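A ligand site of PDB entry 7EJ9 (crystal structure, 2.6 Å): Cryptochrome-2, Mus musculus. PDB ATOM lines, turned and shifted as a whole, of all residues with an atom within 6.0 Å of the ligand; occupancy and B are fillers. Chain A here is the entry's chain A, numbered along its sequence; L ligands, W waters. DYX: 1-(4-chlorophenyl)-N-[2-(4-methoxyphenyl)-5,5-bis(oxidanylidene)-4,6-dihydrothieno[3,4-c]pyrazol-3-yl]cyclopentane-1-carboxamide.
The side-chain hydroxyl (OG) of Ser 416 lies within hydrogen-bond range of the backbone carbonyl oxygen (O) of Val 412 (2.8 Å). ND1 of His 375 sits at hydrogen-bond distance from NE of Arg 378, 3.4 Å away. OD2 of Asp 407 is in salt-bridge range of NH2 of Arg 378 (2.5 Å). O of Leu 275 sits at hydrogen-bond distance from NH2 of Arg 313 (3.3 Å). NE2 of His 375 sits at hydrogen-bond distance from OE1 of Gln 309 (2.8 Å). The indole nitrogen (NE1) of Trp 417 lies close to the side-chain amide oxygen (OD1) of Asn 413 (3.1 Å). The side-chain hydroxyl (OG) of Ser 272 is in hydrogen-bond range of the side-chain carboxylate (OD2) of Asp 407, at 2.6 Å.
OG of Ser 416 is in hydrogen-bond range of N03 of the ligand (2.7 Å). A nitrogen (N07) of the ligand is in hydrogen-bond range of the guanidinium group (NH1) of Arg 378 (2.9 Å). N of Arg 313 lies close to O21 of the ligand (3.4 Å). NE2 of His 375 lies within hydrogen-bond range of O02 of the ligand. O15 of the ligand lies within hydrogen-bond range of NE1 of Trp 417 (3.1 Å). An oxygen (O02) of the ligand is in hydrogen-bond range of the side-chain amide nitrogen (NE2) of Gln 309.
Residues that only touch the ligand: Trp 312 (3.4 Å), Phe 316 (3.4 Å), His 379 (3.4 Å), Ala 382 (3.6 Å), Phe 401 (3.3 Å), Asp 407 (3.1 Å), Ala 408 (3.8 Å), Val 412 (3.5 Å), Asn 413 (3.2 Å), Trp 419 (3.4 Å) and Leu 420 (3.8 Å). Hydrophobic or aromatic side chains that line the ligand: Trp 312, Phe 316, His 375, Ala 382, Phe 401, Ala 408, Val 412, Trp 417, Trp 419 and Leu 420. 17 residues have an atom within 4 Å of the ligand: Gln 309, Trp 312, Arg 313, Phe 316, His 375, Arg 378, His 379, Ala 382, Phe 401, Asp 407, Ala 408, Val 412, Asn 413, Ser 416, Trp 417, Trp 419 and Leu 420. The nearest printed residue that does not touch the ligand is Leu 405 (4.1 Å).
Water W1 lies within hydrogen-bond range of OD2 of Asp 407 (2.9 Å) and NE2 of His 375 (3.2 Å).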
ATOM      1  N   SER A 272       1.005  -9.853 -37.573  1.00  0.00           N
ATOM      2  CA  SER A 272       0.959 -10.909 -36.558  1.00  0.00           C
ATOM      3  C   SER A 272      -0.192 -11.899 -36.766  1.00  0.00           C
ATOM      4  O   SER A 272       0.036 -13.102 -36.602  1.00  0.00           O
ATOM      5  CB  SER A 272       0.916 -10.279 -35.156  1.00  0.00           C
ATOM      6  OG  SER A 272      -0.308  -9.645 -34.865  1.00  0.00           O
ATOM      7  N   LEU A 275       0.998 -14.375 -39.454  1.00  0.00           N
ATOM      8  CA  LEU A 275       1.981 -15.350 -39.002  1.00  0.00           C
ATOM      9  C   LEU A 275       1.306 -16.497 -38.260  1.00  0.00           C
ATOM     10  O   LEU A 275       1.729 -17.653 -38.379  1.00  0.00           O
ATOM     11  CB  LEU A 275       3.033 -14.683 -38.116  1.00  0.00           C
ATOM     12  CG  LEU A 275       4.011 -13.720 -38.780  1.00  0.00           C
ATOM     13  CD1 LEU A 275       4.796 -12.996 -37.715  1.00  0.00           C
ATOM     14  CD2 LEU A 275       4.947 -14.469 -39.719  1.00  0.00           C
ATOM     15  N   GLN A 309      10.072 -10.188 -32.074  1.00  0.00           N
ATOM     16  CA  GLN A 309       8.755 -10.824 -32.067  1.00  0.00           C
ATOM     17  C   GLN A 309       8.810 -12.239 -32.626  1.00  0.00           C
ATOM     18  O   GLN A 309       8.226 -13.164 -32.066  1.00  0.00           O
ATOM     19  CB  GLN A 309       7.766  -9.976 -32.868  1.00  0.00           C
ATOM     20  CG  GLN A 309       7.222  -8.793 -32.105  1.00  0.00           C
ATOM     21  CD  GLN A 309       6.471  -9.210 -30.855  1.00  0.00           C
ATOM     22  OE1 GLN A 309       5.326  -9.646 -30.920  1.00  0.00           O
ATOM     23  NE2 GLN A 309       7.131  -9.067 -29.704  1.00  0.00           N
ATOM     24  N   LEU A 310       9.512 -12.421 -33.751  1.00  0.00           N
ATOM     25  CA  LEU A 310       9.641 -13.758 -34.333  1.00  0.00           C
ATOM     26  C   LEU A 310      10.376 -14.710 -33.385  1.00  0.00           C
ATOM     27  O   LEU A 310      10.055 -15.895 -33.330  1.00  0.00           O
ATOM     28  CB  LEU A 310      10.344 -13.693 -35.678  1.00  0.00           C
ATOM     29  CG  LEU A 310       9.529 -13.187 -36.881  1.00  0.00           C
ATOM     30  CD1 LEU A 310      10.397 -13.139 -38.131  1.00  0.00           C
ATOM     31  CD2 LEU A 310       8.316 -14.062 -37.124  1.00  0.00           C
ATOM     32  N   TRP A 312      10.538 -14.444 -29.950  1.00  0.00           N
ATOM     33  CA  TRP A 312       9.629 -14.793 -28.865  1.00  0.00           C
ATOM     34  C   TRP A 312       8.626 -15.848 -29.315  1.00  0.00           C
ATOM     35  O   TRP A 312       8.368 -16.830 -28.607  1.00  0.00           O
ATOM     36  CB  TRP A 312       8.903 -13.548 -28.351  1.00  0.00           C
ATOM     37  CG  TRP A 312       9.649 -12.811 -27.288  1.00  0.00           C
ATOM     38  CD1 TRP A 312      10.243 -11.581 -27.398  1.00  0.00           C
ATOM     39  CD2 TRP A 312       9.893 -13.242 -25.937  1.00  0.00           C
ATOM     40  NE1 TRP A 312      10.833 -11.224 -26.207  1.00  0.00           N
ATOM     41  CE2 TRP A 312      10.638 -12.227 -25.304  1.00  0.00           C
ATOM     42  CE3 TRP A 312       9.558 -14.398 -25.223  1.00  0.00           C
ATOM     43  CZ2 TRP A 312      11.041 -12.326 -23.977  1.00  0.00           C
ATOM     44  CZ3 TRP A 312       9.971 -14.493 -23.896  1.00  0.00           C
ATOM     45  CH2 TRP A 312      10.698 -13.464 -23.286  1.00  0.00           C
ATOM     46  N   ARG A 313       8.035 -15.651 -30.490  1.00  0.00           N
ATOM     47  CA  ARG A 313       7.246 -16.695 -31.141  1.00  0.00           C
ATOM     48  C   ARG A 313       7.956 -18.037 -31.075  1.00  0.00           C
ATOM     49  O   ARG A 313       7.418 -19.027 -30.579  1.00  0.00           O
ATOM     50  CB  ARG A 313       6.990 -16.296 -32.588  1.00  0.00           C
ATOM     51  CG  ARG A 313       6.005 -17.151 -33.339  1.00  0.00           C
ATOM     52  CD  ARG A 313       5.784 -16.551 -34.730  1.00  0.00           C
ATOM     53  NE  ARG A 313       4.918 -17.362 -35.557  1.00  0.00           N
ATOM     54  CZ  ARG A 313       5.342 -18.301 -36.383  1.00  0.00           C
ATOM     55  NH1 ARG A 313       6.626 -18.601 -36.491  1.00  0.00           N
ATOM     56  NH2 ARG A 313       4.455 -18.979 -37.118  1.00  0.00           N
ATOM     57  N   GLU A 314       9.199 -18.065 -31.577  1.00  0.00           N
ATOM     58  CA  GLU A 314       9.945 -19.311 -31.699  1.00  0.00           C
ATOM     59  C   GLU A 314      10.330 -19.889 -30.338  1.00  0.00           C
ATOM     60  O   GLU A 314      10.367 -21.106 -30.180  1.00  0.00           O
ATOM     61  CB  GLU A 314      11.200 -19.077 -32.543  1.00  0.00           C
ATOM     62  CG  GLU A 314      11.844 -20.336 -33.063  1.00  0.00           C
ATOM     63  CD  GLU A 314      11.356 -20.701 -34.452  1.00  0.00           C
ATOM     64  OE1 GLU A 314      10.491 -19.975 -34.961  1.00  0.00           O
ATOM     65  OE2 GLU A 314      11.854 -21.703 -35.015  1.00  0.00           O
ATOM     66  N   PHE A 316       8.445 -19.632 -27.500  1.00  0.00           N
ATOM     67  CA  PHE A 316       7.250 -20.260 -26.939  1.00  0.00           C
ATOM     68  C   PHE A 316       6.902 -21.567 -27.645  1.00  0.00           C
ATOM     69  O   PHE A 316       6.494 -22.537 -27.002  1.00  0.00           O
ATOM     70  CB  PHE A 316       6.081 -19.289 -26.978  1.00  0.00           C
ATOM     71  CG  PHE A 316       6.214 -18.137 -26.033  1.00  0.00           C
ATOM     72  CD1 PHE A 316       6.718 -18.321 -24.753  1.00  0.00           C
ATOM     73  CD2 PHE A 316       5.854 -16.856 -26.427  1.00  0.00           C
ATOM     74  CE1 PHE A 316       6.842 -17.258 -23.884  1.00  0.00           C
ATOM     75  CE2 PHE A 316       5.988 -15.789 -25.558  1.00  0.00           C
ATOM     76  CZ  PHE A 316       6.479 -15.996 -24.290  1.00  0.00           C
ATOM     77  N   HIS A 375       0.514  -4.909 -27.607  1.00  0.00           N
ATOM     78  CA  HIS A 375       1.179  -5.609 -26.503  1.00  0.00           C
ATOM     79  C   HIS A 375       1.121  -4.805 -25.214  1.00  0.00           C
ATOM     80  O   HIS A 375       0.988  -5.378 -24.124  1.00  0.00           O
ATOM     81  CB  HIS A 375       2.626  -5.936 -26.872  1.00  0.00           C
ATOM     82  CG  HIS A 375       2.778  -7.133 -27.747  1.00  0.00           C
ATOM     83  ND1 HIS A 375       1.740  -8.009 -27.990  1.00  0.00           N
ATOM     84  CD2 HIS A 375       3.836  -7.607 -28.440  1.00  0.00           C
ATOM     85  CE1 HIS A 375       2.163  -8.969 -28.792  1.00  0.00           C
ATOM     86  NE2 HIS A 375       3.425  -8.740 -29.088  1.00  0.00           N
ATOM     87  N   LEU A 376       1.273  -3.489 -25.305  1.00  0.00           N
ATOM     88  CA  LEU A 376       1.038  -2.645 -24.141  1.00  0.00           C
ATOM     89  C   LEU A 376      -0.374  -2.850 -23.592  1.00  0.00           C
ATOM     90  O   LEU A 376      -0.568  -3.048 -22.388  1.00  0.00           O
ATOM     91  CB  LEU A 376       1.274  -1.173 -24.485  1.00  0.00           C
ATOM     92  N   ARG A 378      -2.191  -5.469 -24.044  1.00  0.00           N
ATOM     93  CA  ARG A 378      -2.213  -6.804 -23.459  1.00  0.00           C
ATOM     94  C   ARG A 378      -1.602  -6.796 -22.065  1.00  0.00           C
ATOM     95  O   ARG A 378      -2.123  -7.451 -21.152  1.00  0.00           O
ATOM     96  CB  ARG A 378      -1.467  -7.788 -24.358  1.00  0.00           C
ATOM     97  CG  ARG A 378      -2.013  -7.870 -25.765  1.00  0.00           C
ATOM     98  CD  ARG A 378      -1.261  -8.864 -26.635  1.00  0.00           C
ATOM     99  NE  ARG A 378      -1.555  -8.624 -28.042  1.00  0.00           N
ATOM    100  CZ  ARG A 378      -1.382  -9.505 -29.017  1.00  0.00           C
ATOM    101  NH1 ARG A 378      -0.929 -10.716 -28.774  1.00  0.00           N
ATOM    102  NH2 ARG A 378      -1.673  -9.154 -30.267  1.00  0.00           N
ATOM    103  N   HIS A 379      -0.512  -6.044 -21.879  1.00  0.00           N
ATOM    104  CA  HIS A 379       0.111  -5.924 -20.576  1.00  0.00           C
ATOM    105  C   HIS A 379      -0.883  -5.407 -19.539  1.00  0.00           C
ATOM    106  O   HIS A 379      -1.060  -6.011 -18.482  1.00  0.00           O
ATOM    107  CB  HIS A 379       1.327  -4.992 -20.667  1.00  0.00           C
ATOM    108  CG  HIS A 379       2.107  -4.884 -19.391  1.00  0.00           C
ATOM    109  ND1 HIS A 379       3.263  -5.607 -19.166  1.00  0.00           N
ATOM    110  CD2 HIS A 379       1.900  -4.135 -18.280  1.00  0.00           C
ATOM    111  CE1 HIS A 379       3.738  -5.307 -17.962  1.00  0.00           C
ATOM    112  NE2 HIS A 379       2.930  -4.420 -17.407  1.00  0.00           N
ATOM    113  N   ALA A 380      -1.541  -4.286 -19.837  1.00  0.00           N
ATOM    114  CA  ALA A 380      -2.482  -3.724 -18.890  1.00  0.00           C
ATOM    115  C   ALA A 380      -3.598  -4.710 -18.565  1.00  0.00           C
ATOM    116  O   ALA A 380      -3.972  -4.899 -17.406  1.00  0.00           O
ATOM    117  CB  ALA A 380      -3.076  -2.424 -19.428  1.00  0.00           C
ATOM    118  N   ALA A 382      -3.792  -8.131 -19.126  1.00  0.00           N
ATOM    119  CA  ALA A 382      -3.358  -9.347 -18.440  1.00  0.00           C
ATOM    120  C   ALA A 382      -3.002  -9.048 -16.987  1.00  0.00           C
ATOM    121  O   ALA A 382      -3.238  -9.884 -16.102  1.00  0.00           O
ATOM    122  CB  ALA A 382      -2.181  -9.974 -19.173  1.00  0.00           C
ATOM    123  N   PHE A 401      -8.332 -15.141 -24.455  1.00  0.00           N
ATOM    124  CA  PHE A 401      -7.525 -14.767 -25.614  1.00  0.00           C
ATOM    125  C   PHE A 401      -7.561 -15.831 -26.697  1.00  0.00           C
ATOM    126  O   PHE A 401      -7.398 -15.512 -27.879  1.00  0.00           O
ATOM    127  CB  PHE A 401      -6.068 -14.504 -25.195  1.00  0.00           C
ATOM    128  CG  PHE A 401      -5.838 -13.119 -24.647  1.00  0.00           C
ATOM    129  CD1 PHE A 401      -6.830 -12.447 -23.962  1.00  0.00           C
ATOM    130  CD2 PHE A 401      -4.614 -12.490 -24.832  1.00  0.00           C
ATOM    131  CE1 PHE A 401      -6.614 -11.183 -23.457  1.00  0.00           C
ATOM    132  CE2 PHE A 401      -4.389 -11.222 -24.327  1.00  0.00           C
ATOM    133  CZ  PHE A 401      -5.394 -10.571 -23.640  1.00  0.00           C
ATOM    134  N   LEU A 405      -8.306 -13.549 -29.588  1.00  0.00           N
ATOM    135  CA  LEU A 405      -7.070 -12.960 -30.102  1.00  0.00           C
ATOM    136  C   LEU A 405      -6.562 -13.735 -31.317  1.00  0.00           C
ATOM    137  O   LEU A 405      -6.419 -14.958 -31.278  1.00  0.00           O
ATOM    138  CB  LEU A 405      -6.002 -12.932 -29.016  1.00  0.00           C
ATOM    139  CG  LEU A 405      -4.654 -12.281 -29.360  1.00  0.00           C
ATOM    140  CD1 LEU A 405      -4.798 -10.784 -29.650  1.00  0.00           C
ATOM    141  CD2 LEU A 405      -3.669 -12.534 -28.228  1.00  0.00           C
ATOM    142  N   ASP A 407      -3.585 -13.498 -33.100  1.00  0.00           N
ATOM    143  CA  ASP A 407      -2.180 -13.698 -33.412  1.00  0.00           C
ATOM    144  C   ASP A 407      -1.431 -14.548 -32.383  1.00  0.00           C
ATOM    145  O   ASP A 407      -0.210 -14.430 -32.268  1.00  0.00           O
ATOM    146  CB  ASP A 407      -1.481 -12.345 -33.600  1.00  0.00           C
ATOM    147  CG  ASP A 407      -1.453 -11.489 -32.330  1.00  0.00           C
ATOM    148  OD1 ASP A 407      -1.838 -11.988 -31.249  1.00  0.00           O
ATOM    149  OD2 ASP A 407      -1.033 -10.312 -32.427  1.00  0.00           O
ATOM    150  N   ALA A 408      -2.141 -15.416 -31.645  1.00  0.00           N
ATOM    151  CA  ALA A 408      -1.498 -16.195 -30.603  1.00  0.00           C
ATOM    152  C   ALA A 408      -2.233 -17.521 -30.447  1.00  0.00           C
ATOM    153  O   ALA A 408      -3.402 -17.528 -30.062  1.00  0.00           O
ATOM    154  CB  ALA A 408      -1.468 -15.441 -29.279  1.00  0.00           C
ATOM    155  N   VAL A 412       2.168 -19.595 -27.984  1.00  0.00           N
ATOM    156  CA  VAL A 412       2.448 -18.184 -27.744  1.00  0.00           C
ATOM    157  C   VAL A 412       1.484 -17.586 -26.723  1.00  0.00           C
ATOM    158  O   VAL A 412       1.874 -16.739 -25.915  1.00  0.00           O
ATOM    159  CB  VAL A 412       2.404 -17.406 -29.070  1.00  0.00           C
ATOM    160  CG1 VAL A 412       2.749 -15.943 -28.830  1.00  0.00           C
ATOM    161  CG2 VAL A 412       3.347 -18.029 -30.088  1.00  0.00           C
ATOM    162  N   ASN A 413       0.212 -18.001 -26.727  1.00  0.00           N
ATOM    163  CA  ASN A 413      -0.738 -17.421 -25.789  1.00  0.00           C
ATOM    164  C   ASN A 413      -0.419 -17.841 -24.354  1.00  0.00           C
ATOM    165  O   ASN A 413      -0.309 -16.993 -23.468  1.00  0.00           O
ATOM    166  CB  ASN A 413      -2.162 -17.830 -26.171  1.00  0.00           C
ATOM    167  CG  ASN A 413      -3.213 -16.994 -25.461  1.00  0.00           C
ATOM    168  OD1 ASN A 413      -2.944 -15.863 -25.034  1.00  0.00           O
ATOM    169  ND2 ASN A 413      -4.422 -17.538 -25.336  1.00  0.00           N
ATOM    170  N   ALA A 414      -0.240 -19.150 -24.121  1.00  0.00           N
ATOM    171  CA  ALA A 414       0.054 -19.621 -22.765  1.00  0.00           C
ATOM    172  C   ALA A 414       1.393 -19.081 -22.271  1.00  0.00           C
ATOM    173  O   ALA A 414       1.496 -18.589 -21.138  1.00  0.00           O
ATOM    174  CB  ALA A 414       0.049 -21.157 -22.720  1.00  0.00           C
ATOM    175  N   GLY A 415       2.431 -19.175 -23.107  1.00  0.00           N
ATOM    176  CA  GLY A 415       3.740 -18.676 -22.707  1.00  0.00           C
ATOM    177  C   GLY A 415       3.702 -17.217 -22.303  1.00  0.00           C
ATOM    178  O   GLY A 415       4.233 -16.840 -21.256  1.00  0.00           O
ATOM    179  N   SER A 416       3.057 -16.382 -23.123  1.00  0.00           N
ATOM    180  CA  SER A 416       2.951 -14.955 -22.807  1.00  0.00           C
ATOM    181  C   SER A 416       2.244 -14.736 -21.473  1.00  0.00           C
ATOM    182  O   SER A 416       2.656 -13.888 -20.672  1.00  0.00           O
ATOM    183  CB  SER A 416       2.223 -14.214 -23.923  1.00  0.00           C
ATOM    184  OG  SER A 416       2.954 -14.223 -25.139  1.00  0.00           O
ATOM    185  N   TRP A 417       1.167 -15.494 -21.217  1.00  0.00           N
ATOM    186  CA  TRP A 417       0.420 -15.297 -19.987  1.00  0.00           C
ATOM    187  C   TRP A 417       1.232 -15.716 -18.758  1.00  0.00           C
ATOM    188  O   TRP A 417       1.238 -15.017 -17.749  1.00  0.00           O
ATOM    189  CB  TRP A 417      -0.911 -16.056 -20.051  1.00  0.00           C
ATOM    190  CG  TRP A 417      -2.011 -15.290 -20.729  1.00  0.00           C
ATOM    191  CD1 TRP A 417      -2.407 -15.379 -22.028  1.00  0.00           C
ATOM    192  CD2 TRP A 417      -2.865 -14.316 -20.120  1.00  0.00           C
ATOM    193  NE1 TRP A 417      -3.448 -14.523 -22.275  1.00  0.00           N
ATOM    194  CE2 TRP A 417      -3.751 -13.850 -21.120  1.00  0.00           C
ATOM    195  CE3 TRP A 417      -2.970 -13.781 -18.829  1.00  0.00           C
ATOM    196  CZ2 TRP A 417      -4.725 -12.891 -20.865  1.00  0.00           C
ATOM    197  CZ3 TRP A 417      -3.941 -12.830 -18.581  1.00  0.00           C
ATOM    198  CH2 TRP A 417      -4.807 -12.387 -19.592  1.00  0.00           C
ATOM    199  N   TRP A 419       4.463 -15.775 -18.644  1.00  0.00           N
ATOM    200  CA  TRP A 419       5.491 -14.742 -18.554  1.00  0.00           C
ATOM    201  C   TRP A 419       4.945 -13.512 -17.846  1.00  0.00           C
ATOM    202  O   TRP A 419       5.543 -13.023 -16.884  1.00  0.00           O
ATOM    203  CB  TRP A 419       5.982 -14.397 -19.966  1.00  0.00           C
ATOM    204  CG  TRP A 419       7.047 -13.341 -20.014  1.00  0.00           C
ATOM    205  CD1 TRP A 419       8.399 -13.527 -19.935  1.00  0.00           C
ATOM    206  CD2 TRP A 419       6.838 -11.928 -20.173  1.00  0.00           C
ATOM    207  NE1 TRP A 419       9.047 -12.319 -20.029  1.00  0.00           N
ATOM    208  CE2 TRP A 419       8.114 -11.325 -20.177  1.00  0.00           C
ATOM    209  CE3 TRP A 419       5.713 -11.119 -20.308  1.00  0.00           C
ATOM    210  CZ2 TRP A 419       8.290  -9.941 -20.305  1.00  0.00           C
ATOM    211  CZ3 TRP A 419       5.888  -9.759 -20.440  1.00  0.00           C
ATOM    212  CH2 TRP A 419       7.155  -9.182 -20.433  1.00  0.00           C
ATOM    213  N   LEU A 420       3.796 -13.007 -18.295  1.00  0.00           N
ATOM    214  CA  LEU A 420       3.238 -11.788 -17.707  1.00  0.00           C
ATOM    215  C   LEU A 420       2.926 -11.984 -16.226  1.00  0.00           C
ATOM    216  O   LEU A 420       3.212 -11.095 -15.401  1.00  0.00           O
ATOM    217  CB  LEU A 420       1.994 -11.353 -18.482  1.00  0.00           C
ATOM    218  CG  LEU A 420       1.356  -9.987 -18.210  1.00  0.00           C
ATOM    219  CD1 LEU A 420       0.502  -9.989 -16.943  1.00  0.00           C
ATOM    220  CD2 LEU A 420       2.413  -8.898 -18.140  1.00  0.00           C
HETATM  221  C10 DYX L   1      -0.138 -13.389 -26.429  1.00  0.00           C
HETATM  222  C13 DYX L   1       0.268 -11.335 -24.569  1.00  0.00           C
HETATM  223  C17 DYX L   1       2.345 -12.843 -31.521  1.00  0.00           C
HETATM  224  C22 DYX L   1       5.724 -11.147 -25.478  1.00  0.00           C
HETATM  225  C24 DYX L   1       7.781 -10.653 -24.337  1.00  0.00           C
HETATM  226  C26 DYX L   1       6.392 -12.486 -24.878  1.00  0.00           C
HETATM  227  C28 DYX L   1       4.028  -9.364 -24.797  1.00  0.00           C
HETATM  228  C01 DYX L   1       4.939 -11.326 -26.803  1.00  0.00           C
HETATM  229  C04 DYX L   1       2.914 -12.419 -27.940  1.00  0.00           C
HETATM  230  C05 DYX L   1       3.308 -12.547 -29.299  1.00  0.00           C
HETATM  231  C06 DYX L   1       2.199 -12.691 -30.016  1.00  0.00           C
HETATM  232  C09 DYX L   1       0.829 -12.404 -26.661  1.00  0.00           C
HETATM  233  C11 DYX L   1      -0.907 -13.349 -25.267  1.00  0.00           C
HETATM  234  C12 DYX L   1      -0.708 -12.324 -24.337  1.00  0.00           C
HETATM  235  C14 DYX L   1       1.028 -11.379 -25.731  1.00  0.00           C
HETATM  236  C16 DYX L   1      -0.818 -11.741 -22.054  1.00  0.00           C
HETATM  237  C19 DYX L   1       4.628 -12.554 -30.059  1.00  0.00           C
HETATM  238  C23 DYX L   1       6.712 -10.271 -25.577  1.00  0.00           C
HETATM  239  C25 DYX L   1       7.481 -11.917 -23.896  1.00  0.00           C
HETATM  240  C27 DYX L   1       4.604 -10.600 -24.501  1.00  0.00           C
HETATM  241  C29 DYX L   1       3.022  -8.845 -23.974  1.00  0.00           C
HETATM  242  C30 DYX L   1       2.605  -9.565 -22.861  1.00  0.00           C
HETATM  243  C31 DYX L   1       3.174 -10.811 -22.571  1.00  0.00           C
HETATM  244  C32 DYX L   1       4.180 -11.330 -23.394  1.00  0.00           C
HETATM  245  N03 DYX L   1       3.776 -12.208 -26.761  1.00  0.00           N
HETATM  246  N07 DYX L   1       1.129 -12.667 -29.129  1.00  0.00           N
HETATM  247  N08 DYX L   1       1.631 -12.477 -27.898  1.00  0.00           N
HETATM  248  O02 DYX L   1       5.254 -10.729 -27.774  1.00  0.00           O
HETATM  249  O15 DYX L   1      -1.481 -12.299 -23.159  1.00  0.00           O
HETATM  250  O20 DYX L   1       4.281 -13.154 -33.115  1.00  0.00           O
HETATM  251  O21 DYX L   1       4.943 -14.509 -31.467  1.00  0.00           O
HETATM  252  S18 DYX L   1       4.119 -13.319 -31.666  1.00  0.00           S
HETATM  253 CL1  DYX L   1       1.334  -8.889 -21.813  1.00  0.00          CL
HETATM  254  O   HOH W   1       1.641  -9.443 -31.628  1.00  0.00           O
